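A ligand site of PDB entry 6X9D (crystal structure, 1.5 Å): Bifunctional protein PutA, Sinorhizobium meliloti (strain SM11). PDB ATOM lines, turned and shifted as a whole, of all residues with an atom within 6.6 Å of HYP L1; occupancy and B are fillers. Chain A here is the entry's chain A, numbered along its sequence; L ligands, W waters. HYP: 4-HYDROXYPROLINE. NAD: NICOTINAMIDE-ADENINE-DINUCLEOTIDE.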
ATOM      1  N   GLU A 676      -5.472  12.582   4.809  1.00  0.00           N
ATOM      2  CA  GLU A 676      -5.846  13.121   3.507  1.00  0.00           C
ATOM      3  C   GLU A 676      -5.127  12.392   2.377  1.00  0.00           C
ATOM      4  O   GLU A 676      -5.713  12.138   1.317  1.00  0.00           O
ATOM      5  CB  GLU A 676      -5.565  14.632   3.455  1.00  0.00           C
ATOM      6  CG  GLU A 676      -6.004  15.269   2.123  1.00  0.00           C
ATOM      7  CD  GLU A 676      -6.320  16.750   2.243  1.00  0.00           C
ATOM      8  OE1 GLU A 676      -7.441  17.081   2.676  1.00  0.00           O
ATOM      9  OE2 GLU A 676      -5.471  17.593   1.892  1.00  0.00           O
ATOM     10  N   PHE A 680      -7.105  10.585  -0.585  1.00  0.00           N
ATOM     11  CA  PHE A 680      -6.819  10.785  -2.007  1.00  0.00           C
ATOM     12  C   PHE A 680      -6.610   9.465  -2.749  1.00  0.00           C
ATOM     13  O   PHE A 680      -7.229   9.209  -3.782  1.00  0.00           O
ATOM     14  CB  PHE A 680      -5.579  11.667  -2.198  1.00  0.00           C
ATOM     15  CG  PHE A 680      -5.836  13.151  -2.104  1.00  0.00           C
ATOM     16  CD1 PHE A 680      -6.823  13.776  -2.853  1.00  0.00           C
ATOM     17  CD2 PHE A 680      -5.042  13.943  -1.265  1.00  0.00           C
ATOM     18  CE1 PHE A 680      -7.044  15.148  -2.770  1.00  0.00           C
ATOM     19  CE2 PHE A 680      -5.244  15.323  -1.176  1.00  0.00           C
ATOM     20  CZ  PHE A 680      -6.246  15.936  -1.923  1.00  0.00           C
ATOM     21  N   ASN A 709       3.547  23.001   2.186  1.00  0.00           N
ATOM     22  CA  ASN A 709       2.702  23.100   3.379  1.00  0.00           C
ATOM     23  C   ASN A 709       1.750  21.926   3.543  1.00  0.00           C
ATOM     24  O   ASN A 709       1.242  21.730   4.648  1.00  0.00           O
ATOM     25  CB  ASN A 709       1.920  24.414   3.360  1.00  0.00           C
ATOM     26  CG  ASN A 709       0.909  24.487   2.241  1.00  0.00           C
ATOM     27  OD1 ASN A 709       1.203  24.170   1.093  1.00  0.00           O
ATOM     28  ND2 ASN A 709      -0.295  24.931   2.574  1.00  0.00           N
ATOM     29  N   PHE A 710       1.509  21.150   2.496  1.00  0.00           N
ATOM     30  CA  PHE A 710       0.870  19.847   2.617  1.00  0.00           C
ATOM     31  C   PHE A 710       1.790  18.861   1.931  1.00  0.00           C
ATOM     32  O   PHE A 710       1.514  18.385   0.831  1.00  0.00           O
ATOM     33  CB  PHE A 710      -0.547  19.836   2.037  1.00  0.00           C
ATOM     34  CG  PHE A 710      -1.482  20.779   2.745  1.00  0.00           C
ATOM     35  CD1 PHE A 710      -1.928  20.491   4.029  1.00  0.00           C
ATOM     36  CD2 PHE A 710      -1.861  21.964   2.154  1.00  0.00           C
ATOM     37  CE1 PHE A 710      -2.781  21.372   4.703  1.00  0.00           C
ATOM     38  CE2 PHE A 710      -2.709  22.838   2.822  1.00  0.00           C
ATOM     39  CZ  PHE A 710      -3.155  22.548   4.093  1.00  0.00           C
ATOM     40  N   ALA A 713       0.079  15.165   1.643  1.00  0.00           N
ATOM     41  CA  ALA A 713      -1.270  14.992   1.121  1.00  0.00           C
ATOM     42  C   ALA A 713      -1.381  15.488  -0.316  1.00  0.00           C
ATOM     43  O   ALA A 713      -1.811  14.745  -1.208  1.00  0.00           O
ATOM     44  CB  ALA A 713      -2.262  15.705   2.021  1.00  0.00           C
ATOM     45  N   ILE A 714      -1.053  16.754  -0.549  1.00  0.00           N
ATOM     46  CA  ILE A 714      -1.196  17.301  -1.897  1.00  0.00           C
ATOM     47  C   ILE A 714      -0.181  16.670  -2.840  1.00  0.00           C
ATOM     48  O   ILE A 714      -0.474  16.403  -4.011  1.00  0.00           O
ATOM     49  CB  ILE A 714      -1.080  18.838  -1.870  1.00  0.00           C
ATOM     50  CG1 ILE A 714      -2.366  19.404  -1.254  1.00  0.00           C
ATOM     51  CG2 ILE A 714      -0.879  19.425  -3.277  1.00  0.00           C
ATOM     52  CD1 ILE A 714      -2.448  20.911  -1.269  1.00  0.00           C
ATOM     53  N   ARG A 845      -1.909  27.129   5.856  1.00  0.00           N
ATOM     54  CA  ARG A 845      -2.825  26.409   4.989  1.00  0.00           C
ATOM     55  C   ARG A 845      -3.295  27.376   3.908  1.00  0.00           C
ATOM     56  O   ARG A 845      -3.523  28.551   4.187  1.00  0.00           O
ATOM     57  CB  ARG A 845      -4.047  25.881   5.747  1.00  0.00           C
ATOM     58  CG  ARG A 845      -3.761  24.841   6.831  1.00  0.00           C
ATOM     59  CD  ARG A 845      -5.106  24.437   7.443  1.00  0.00           C
ATOM     60  NE  ARG A 845      -4.926  23.393   8.442  1.00  0.00           N
ATOM     61  CZ  ARG A 845      -5.137  22.105   8.232  1.00  0.00           C
ATOM     62  NH1 ARG A 845      -5.550  21.664   7.045  1.00  0.00           N
ATOM     63  NH2 ARG A 845      -4.931  21.254   9.216  1.00  0.00           N
ATOM     64  N   CYS A 846      -3.454  26.880   2.682  1.00  0.00           N
ATOM     65  CA  CYS A 846      -4.015  27.741   1.653  1.00  0.00           C
ATOM     66  C   CYS A 846      -5.443  28.165   1.999  1.00  0.00           C
ATOM     67  O   CYS A 846      -5.886  29.239   1.577  1.00  0.00           O
ATOM     68  CB  CYS A 846      -3.983  27.036   0.305  1.00  0.00           C
ATOM     69  SG  CYS A 846      -4.709  25.379   0.352  1.00  0.00           S
ATOM     70  N   SER A 847      -6.146  27.348   2.779  1.00  0.00           N
ATOM     71  CA  SER A 847      -7.518  27.561   3.212  1.00  0.00           C
ATOM     72  C   SER A 847      -7.637  28.478   4.427  1.00  0.00           C
ATOM     73  O   SER A 847      -8.759  28.777   4.844  1.00  0.00           O
ATOM     74  CB  SER A 847      -8.141  26.201   3.576  1.00  0.00           C
ATOM     75  OG  SER A 847      -7.238  25.517   4.432  1.00  0.00           O
ATOM     76  N   ALA A 848      -6.522  28.924   4.991  1.00  0.00           N
ATOM     77  CA  ALA A 848      -6.537  29.601   6.281  1.00  0.00           C
ATOM     78  C   ALA A 848      -7.333  30.894   6.221  1.00  0.00           C
ATOM     79  O   ALA A 848      -7.380  31.585   5.191  1.00  0.00           O
ATOM     80  CB  ALA A 848      -5.102  29.901   6.740  1.00  0.00           C
ATOM     81  N   THR A 973     -11.447  29.602  -0.019  1.00  0.00           N
ATOM     82  CA  THR A 973     -12.373  29.236   1.043  1.00  0.00           C
ATOM     83  C   THR A 973     -13.087  30.476   1.562  1.00  0.00           C
ATOM     84  O   THR A 973     -12.593  31.606   1.438  1.00  0.00           O
ATOM     85  CB  THR A 973     -11.680  28.515   2.212  1.00  0.00           C
ATOM     86  OG1 THR A 973     -10.666  29.365   2.757  1.00  0.00           O
ATOM     87  CG2 THR A 973     -11.063  27.195   1.761  1.00  0.00           C
ATOM     88  N   TYR A 997     -18.238  27.431   3.932  1.00  0.00           N
ATOM     89  CA  TYR A 997     -18.393  26.770   5.220  1.00  0.00           C
ATOM     90  C   TYR A 997     -19.356  27.586   6.073  1.00  0.00           C
ATOM     91  O   TYR A 997     -19.143  28.785   6.250  1.00  0.00           O
ATOM     92  CB  TYR A 997     -17.049  26.645   5.937  1.00  0.00           C
ATOM     93  CG  TYR A 997     -16.043  25.832   5.150  1.00  0.00           C
ATOM     94  CD1 TYR A 997     -16.014  24.451   5.253  1.00  0.00           C
ATOM     95  CD2 TYR A 997     -15.161  26.456   4.274  1.00  0.00           C
ATOM     96  CE1 TYR A 997     -15.114  23.700   4.535  1.00  0.00           C
ATOM     97  CE2 TYR A 997     -14.247  25.701   3.536  1.00  0.00           C
ATOM     98  CZ  TYR A 997     -14.232  24.327   3.673  1.00  0.00           C
ATOM     99  OH  TYR A 997     -13.343  23.556   2.951  1.00  0.00           O
ATOM    100  N   ILE A1002     -13.087  26.874   8.420  1.00  0.00           N
ATOM    101  CA  ILE A1002     -12.957  26.894   6.959  1.00  0.00           C
ATOM    102  C   ILE A1002     -11.758  26.083   6.494  1.00  0.00           C
ATOM    103  O   ILE A1002     -11.326  26.224   5.338  1.00  0.00           O
ATOM    104  CB  ILE A1002     -12.934  28.335   6.401  1.00  0.00           C
ATOM    105  CG1 ILE A1002     -11.640  29.082   6.772  1.00  0.00           C
ATOM    106  CG2 ILE A1002     -14.168  29.094   6.881  1.00  0.00           C
ATOM    107  CD1 ILE A1002     -11.471  30.422   5.997  1.00  0.00           C
ATOM    108  N   ILE A1003     -11.209  25.215   7.344  1.00  0.00           N
ATOM    109  CA  ILE A1003     -10.004  24.477   7.009  1.00  0.00           C
ATOM    110  C   ILE A1003     -10.288  22.984   7.036  1.00  0.00           C
ATOM    111  O   ILE A1003     -11.325  22.527   7.511  1.00  0.00           O
ATOM    112  CB  ILE A1003      -8.827  24.805   7.946  1.00  0.00           C
ATOM    113  CG1 ILE A1003      -9.189  24.479   9.402  1.00  0.00           C
ATOM    114  CG2 ILE A1003      -8.372  26.240   7.760  1.00  0.00           C
ATOM    115  CD1 ILE A1003      -7.953  24.419  10.323  1.00  0.00           C
ATOM    116  N   GLY A1004      -9.332  22.217   6.527  1.00  0.00           N
ATOM    117  CA  GLY A1004      -9.436  20.776   6.590  1.00  0.00           C
ATOM    118  C   GLY A1004     -10.510  20.175   5.712  1.00  0.00           C
ATOM    119  O   GLY A1004     -11.193  19.242   6.134  1.00  0.00           O
ATOM    120  N   ALA A1005     -10.683  20.711   4.495  1.00  0.00           N
ATOM    121  CA  ALA A1005     -11.592  20.085   3.538  1.00  0.00           C
ATOM    122  C   ALA A1005     -11.233  18.622   3.344  1.00  0.00           C
ATOM    123  O   ALA A1005     -10.063  18.261   3.202  1.00  0.00           O
ATOM    124  CB  ALA A1005     -11.540  20.806   2.182  1.00  0.00           C
ATOM    125  N   VAL A1006     -12.268  17.776   3.310  1.00  0.00           N
ATOM    126  CA  VAL A1006     -12.132  16.329   3.316  1.00  0.00           C
ATOM    127  C   VAL A1006     -12.370  15.799   1.904  1.00  0.00           C
ATOM    128  O   VAL A1006     -13.362  16.150   1.266  1.00  0.00           O
ATOM    129  CB  VAL A1006     -13.126  15.698   4.303  1.00  0.00           C
ATOM    130  CG1 VAL A1006     -13.143  14.183   4.155  1.00  0.00           C
ATOM    131  CG2 VAL A1006     -12.759  16.113   5.731  1.00  0.00           C
ATOM    132  N   VAL A1007     -11.467  14.929   1.455  1.00  0.00           N
ATOM    133  CA  VAL A1007     -11.555  14.361   0.110  1.00  0.00           C
ATOM    134  C   VAL A1007     -12.920  13.707  -0.097  1.00  0.00           C
ATOM    135  O   VAL A1007     -13.382  12.929   0.733  1.00  0.00           O
ATOM    136  CB  VAL A1007     -10.407  13.369  -0.092  1.00  0.00           C
ATOM    137  CG1 VAL A1007     -10.572  12.627  -1.401  1.00  0.00           C
ATOM    138  CG2 VAL A1007      -9.078  14.095  -0.075  1.00  0.00           C
ATOM    139  N   GLN A1010     -15.823  17.533   0.990  1.00  0.00           N
ATOM    140  CA  GLN A1010     -15.697  18.896   0.489  1.00  0.00           C
ATOM    141  C   GLN A1010     -14.605  18.885  -0.585  1.00  0.00           C
ATOM    142  O   GLN A1010     -13.456  19.253  -0.307  1.00  0.00           O
ATOM    143  CB  GLN A1010     -15.353  19.906   1.590  1.00  0.00           C
ATOM    144  CG  GLN A1010     -16.336  19.920   2.771  1.00  0.00           C
ATOM    145  CD  GLN A1010     -15.919  19.030   3.927  1.00  0.00           C
ATOM    146  OE1 GLN A1010     -14.721  18.791   4.159  1.00  0.00           O
ATOM    147  NE2 GLN A1010     -16.907  18.561   4.688  1.00  0.00           N
ATOM    148  N   PHE A1012     -12.115  20.116  -3.021  1.00  0.00           N
ATOM    149  CA  PHE A1012     -11.400  21.330  -2.651  1.00  0.00           C
ATOM    150  C   PHE A1012     -10.820  22.026  -3.869  1.00  0.00           C
ATOM    151  O   PHE A1012     -10.104  21.403  -4.666  1.00  0.00           O
ATOM    152  CB  PHE A1012     -10.284  21.041  -1.663  1.00  0.00           C
ATOM    153  CG  PHE A1012      -9.627  22.282  -1.143  1.00  0.00           C
ATOM    154  CD1 PHE A1012     -10.253  23.039  -0.165  1.00  0.00           C
ATOM    155  CD2 PHE A1012      -8.394  22.696  -1.648  1.00  0.00           C
ATOM    156  CE1 PHE A1012      -9.671  24.191   0.310  1.00  0.00           C
ATOM    157  CE2 PHE A1012      -7.800  23.850  -1.165  1.00  0.00           C
ATOM    158  CZ  PHE A1012      -8.430  24.596  -0.178  1.00  0.00           C
ATOM    159  N   ALA A1024      -9.353  19.158  -6.806  1.00  0.00           N
ATOM    160  CA  ALA A1024      -8.796  17.979  -6.163  1.00  0.00           C
ATOM    161  C   ALA A1024      -9.819  17.382  -5.206  1.00  0.00           C
ATOM    162  O   ALA A1024     -10.587  18.087  -4.551  1.00  0.00           O
ATOM    163  CB  ALA A1024      -7.519  18.339  -5.392  1.00  0.00           C
HETATM  164  N   HYP L   1      -7.582  19.999   2.478  1.00  0.00           N
HETATM  165  CA  HYP L   1      -6.709  20.997   3.152  1.00  0.00           C
HETATM  166  C   HYP L   1      -7.529  22.192   3.796  1.00  0.00           C
HETATM  167  O   HYP L   1      -6.933  22.807   4.715  1.00  0.00           O
HETATM  168  CB  HYP L   1      -5.720  21.479   2.092  1.00  0.00           C
HETATM  169  CG  HYP L   1      -6.281  20.964   0.745  1.00  0.00           C
HETATM  170  CD  HYP L   1      -7.711  20.490   1.084  1.00  0.00           C
HETATM  171  OD1 HYP L   1      -5.477  19.880   0.310  1.00  0.00           O
HETATM  172  OXT HYP L   1      -8.683  22.436   3.399  1.00  0.00           O
HETATM  173  PA  NAD L   2       5.555  28.003  -4.269  1.00  0.00           P
HETATM  174  O1A NAD L   2       4.875  28.730  -5.380  1.00  0.00           O
HETATM  175  O2A NAD L   2       6.624  28.870  -3.681  1.00  0.00           O
HETATM  176  O5B NAD L   2       6.227  26.586  -4.806  1.00  0.00           O
HETATM  177  C5B NAD L   2       5.417  25.441  -5.073  1.00  0.00           C
HETATM  178  C4B NAD L   2       6.295  24.502  -5.957  1.00  0.00           C
HETATM  179  O4B NAD L   2       6.694  25.302  -7.293  1.00  0.00           O
HETATM  180  C3B NAD L   2       7.422  24.151  -5.383  1.00  0.00           C
HETATM  181  O3B NAD L   2       7.634  22.678  -5.583  1.00  0.00           O
HETATM  182  C2B NAD L   2       8.538  24.968  -6.081  1.00  0.00           C
HETATM  183  O2B NAD L   2       9.737  24.300  -6.025  1.00  0.00           O
HETATM  184  C1B NAD L   2       7.995  25.125  -7.492  1.00  0.00           C
HETATM  185  N9A NAD L   2       8.501  26.327  -8.121  1.00  0.00           N
HETATM  186  C8A NAD L   2       8.955  27.506  -7.716  1.00  0.00           C
HETATM  187  N7A NAD L   2       9.251  28.202  -8.836  1.00  0.00           N
HETATM  188  C5A NAD L   2       8.962  27.434  -9.917  1.00  0.00           C
HETATM  189  C6A NAD L   2       9.084  27.671 -11.290  1.00  0.00           C
HETATM  190  N6A NAD L   2       9.595  28.961 -11.805  1.00  0.00           N
HETATM  191  N1A NAD L   2       8.720  26.730 -12.154  1.00  0.00           N
HETATM  192  C2A NAD L   2       8.239  25.525 -11.696  1.00  0.00           C
HETATM  193  N3A NAD L   2       8.124  25.290 -10.374  1.00  0.00           N
HETATM  194  C4A NAD L   2       8.488  26.266  -9.481  1.00  0.00           C
HETATM  195  O3  NAD L   2       4.415  27.659  -3.130  1.00  0.00           O
HETATM  196  PN  NAD L   2       4.643  27.042  -1.590  1.00  0.00           P
HETATM  197  O1N NAD L   2       5.420  28.083  -0.764  1.00  0.00           O
HETATM  198  O2N NAD L   2       5.331  25.697  -1.614  1.00  0.00           O
HETATM  199  O5D NAD L   2       3.137  26.930  -0.950  1.00  0.00           O
HETATM  200  C5D NAD L   2       2.513  28.151  -0.581  1.00  0.00           C
HETATM  201  C4D NAD L   2       1.490  28.642  -1.609  1.00  0.00           C
HETATM  202  O4D NAD L   2       0.681  27.379  -2.177  1.00  0.00           O
HETATM  203  C3D NAD L   2       0.586  29.460  -1.063  1.00  0.00           C
HETATM  204  O3D NAD L   2       0.314  30.629  -2.005  1.00  0.00           O
HETATM  205  C2D NAD L   2      -0.664  28.637  -0.899  1.00  0.00           C
HETATM  206  O2D NAD L   2      -1.834  29.405  -0.907  1.00  0.00           O
HETATM  207  C1D NAD L   2      -0.556  27.728  -2.166  1.00  0.00           C
HETATM  208  N1N NAD L   2      -1.402  26.523  -1.947  1.00  0.00           N
HETATM  209  C2N NAD L   2      -2.578  26.350  -2.661  1.00  0.00           C
HETATM  210  C3N NAD L   2      -3.323  25.216  -2.406  1.00  0.00           C
HETATM  211  C7N NAD L   2      -4.663  24.938  -3.168  1.00  0.00           C
HETATM  212  O7N NAD L   2      -5.152  23.858  -3.117  1.00  0.00           O
HETATM  213  N7N NAD L   2      -5.313  26.045  -3.911  1.00  0.00           N
HETATM  214  C4N NAD L   2      -2.874  24.271  -1.512  1.00  0.00           C
HETATM  215  C5N NAD L   2      -1.729  24.469  -0.783  1.00  0.00           C
HETATM  216  C6N NAD L   2      -0.988  25.610  -1.032  1.00  0.00           C
HETATM  217  O   HOH W   1      -9.111  17.578   0.721  1.00  0.00           O
HETATM  218  O   HOH W   2     -10.920  24.166   3.517  1.00  0.00           O
HETATM  219  O   HOH W   3      -6.078  19.383  -2.285  1.00  0.00           O
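An oxygen (O) of HYP L1 is in hydrogen-bond range of the side-chain hydroxyl (OG) of Ser 847 (2.7 Å).
OE1 of Glu 676 lies within salt-bridge range of N of HYP L1, 2.9 Å away.
N of Ala 1005 sits at hydrogen-bond distance from OXT of HYP L1, at 2.9 Å.
O of Ala 1005 is in hydrogen-bond range of N of HYP L1 (3.1 Å).
The guanidinium group (NH1) of Arg 845 lies within salt-bridge range of an oxygen (O) of HYP L1 (2.9 Å).
O of HYP L1 lies within hydrogen-bond range of N of Gly 1004.
OG1 of Thr 973 is in hydrogen-bond range of O of Ser 847 (2.9 Å).
N of Phe 1012 lies within hydrogen-bond range of O of Ala 1024, 3.0 Å away.
CE2 of Phe 710 touches CB of HYP L1, 3.4 Å away.
CG1 of Ile 714 touches OD1 of HYP L1, at 3.5 Å.
Phe 1012 touches HYP L1 (CG to CD, 3.4 Å).
Hydrophobic or aromatic side chains within 4 Å of HYP L1: Phe 710, Ile 714, Ala 1005 and Phe 1012.
Eight residues have an atom within 4 Å of HYP L1: Glu 676, Phe 710, Ile 714, Arg 845, Ser 847, Gly 1004, Ala 1005 and Phe 1012.
Water W2 lies within hydrogen-bond range of OH of Tyr 997 (2.6 Å), O of Ile 1002 (2.8 Å) and OXT of HYP L1 (2.8 Å).
Water W1 lies within hydrogen-bond range of the side-chain carboxylate (OE1) of Glu 676 (2.6 Å), the backbone carbonyl oxygen (O) of Ala 1005 (2.7 Å) and a nitrogen (N) of HYP L1 (3.4 Å).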
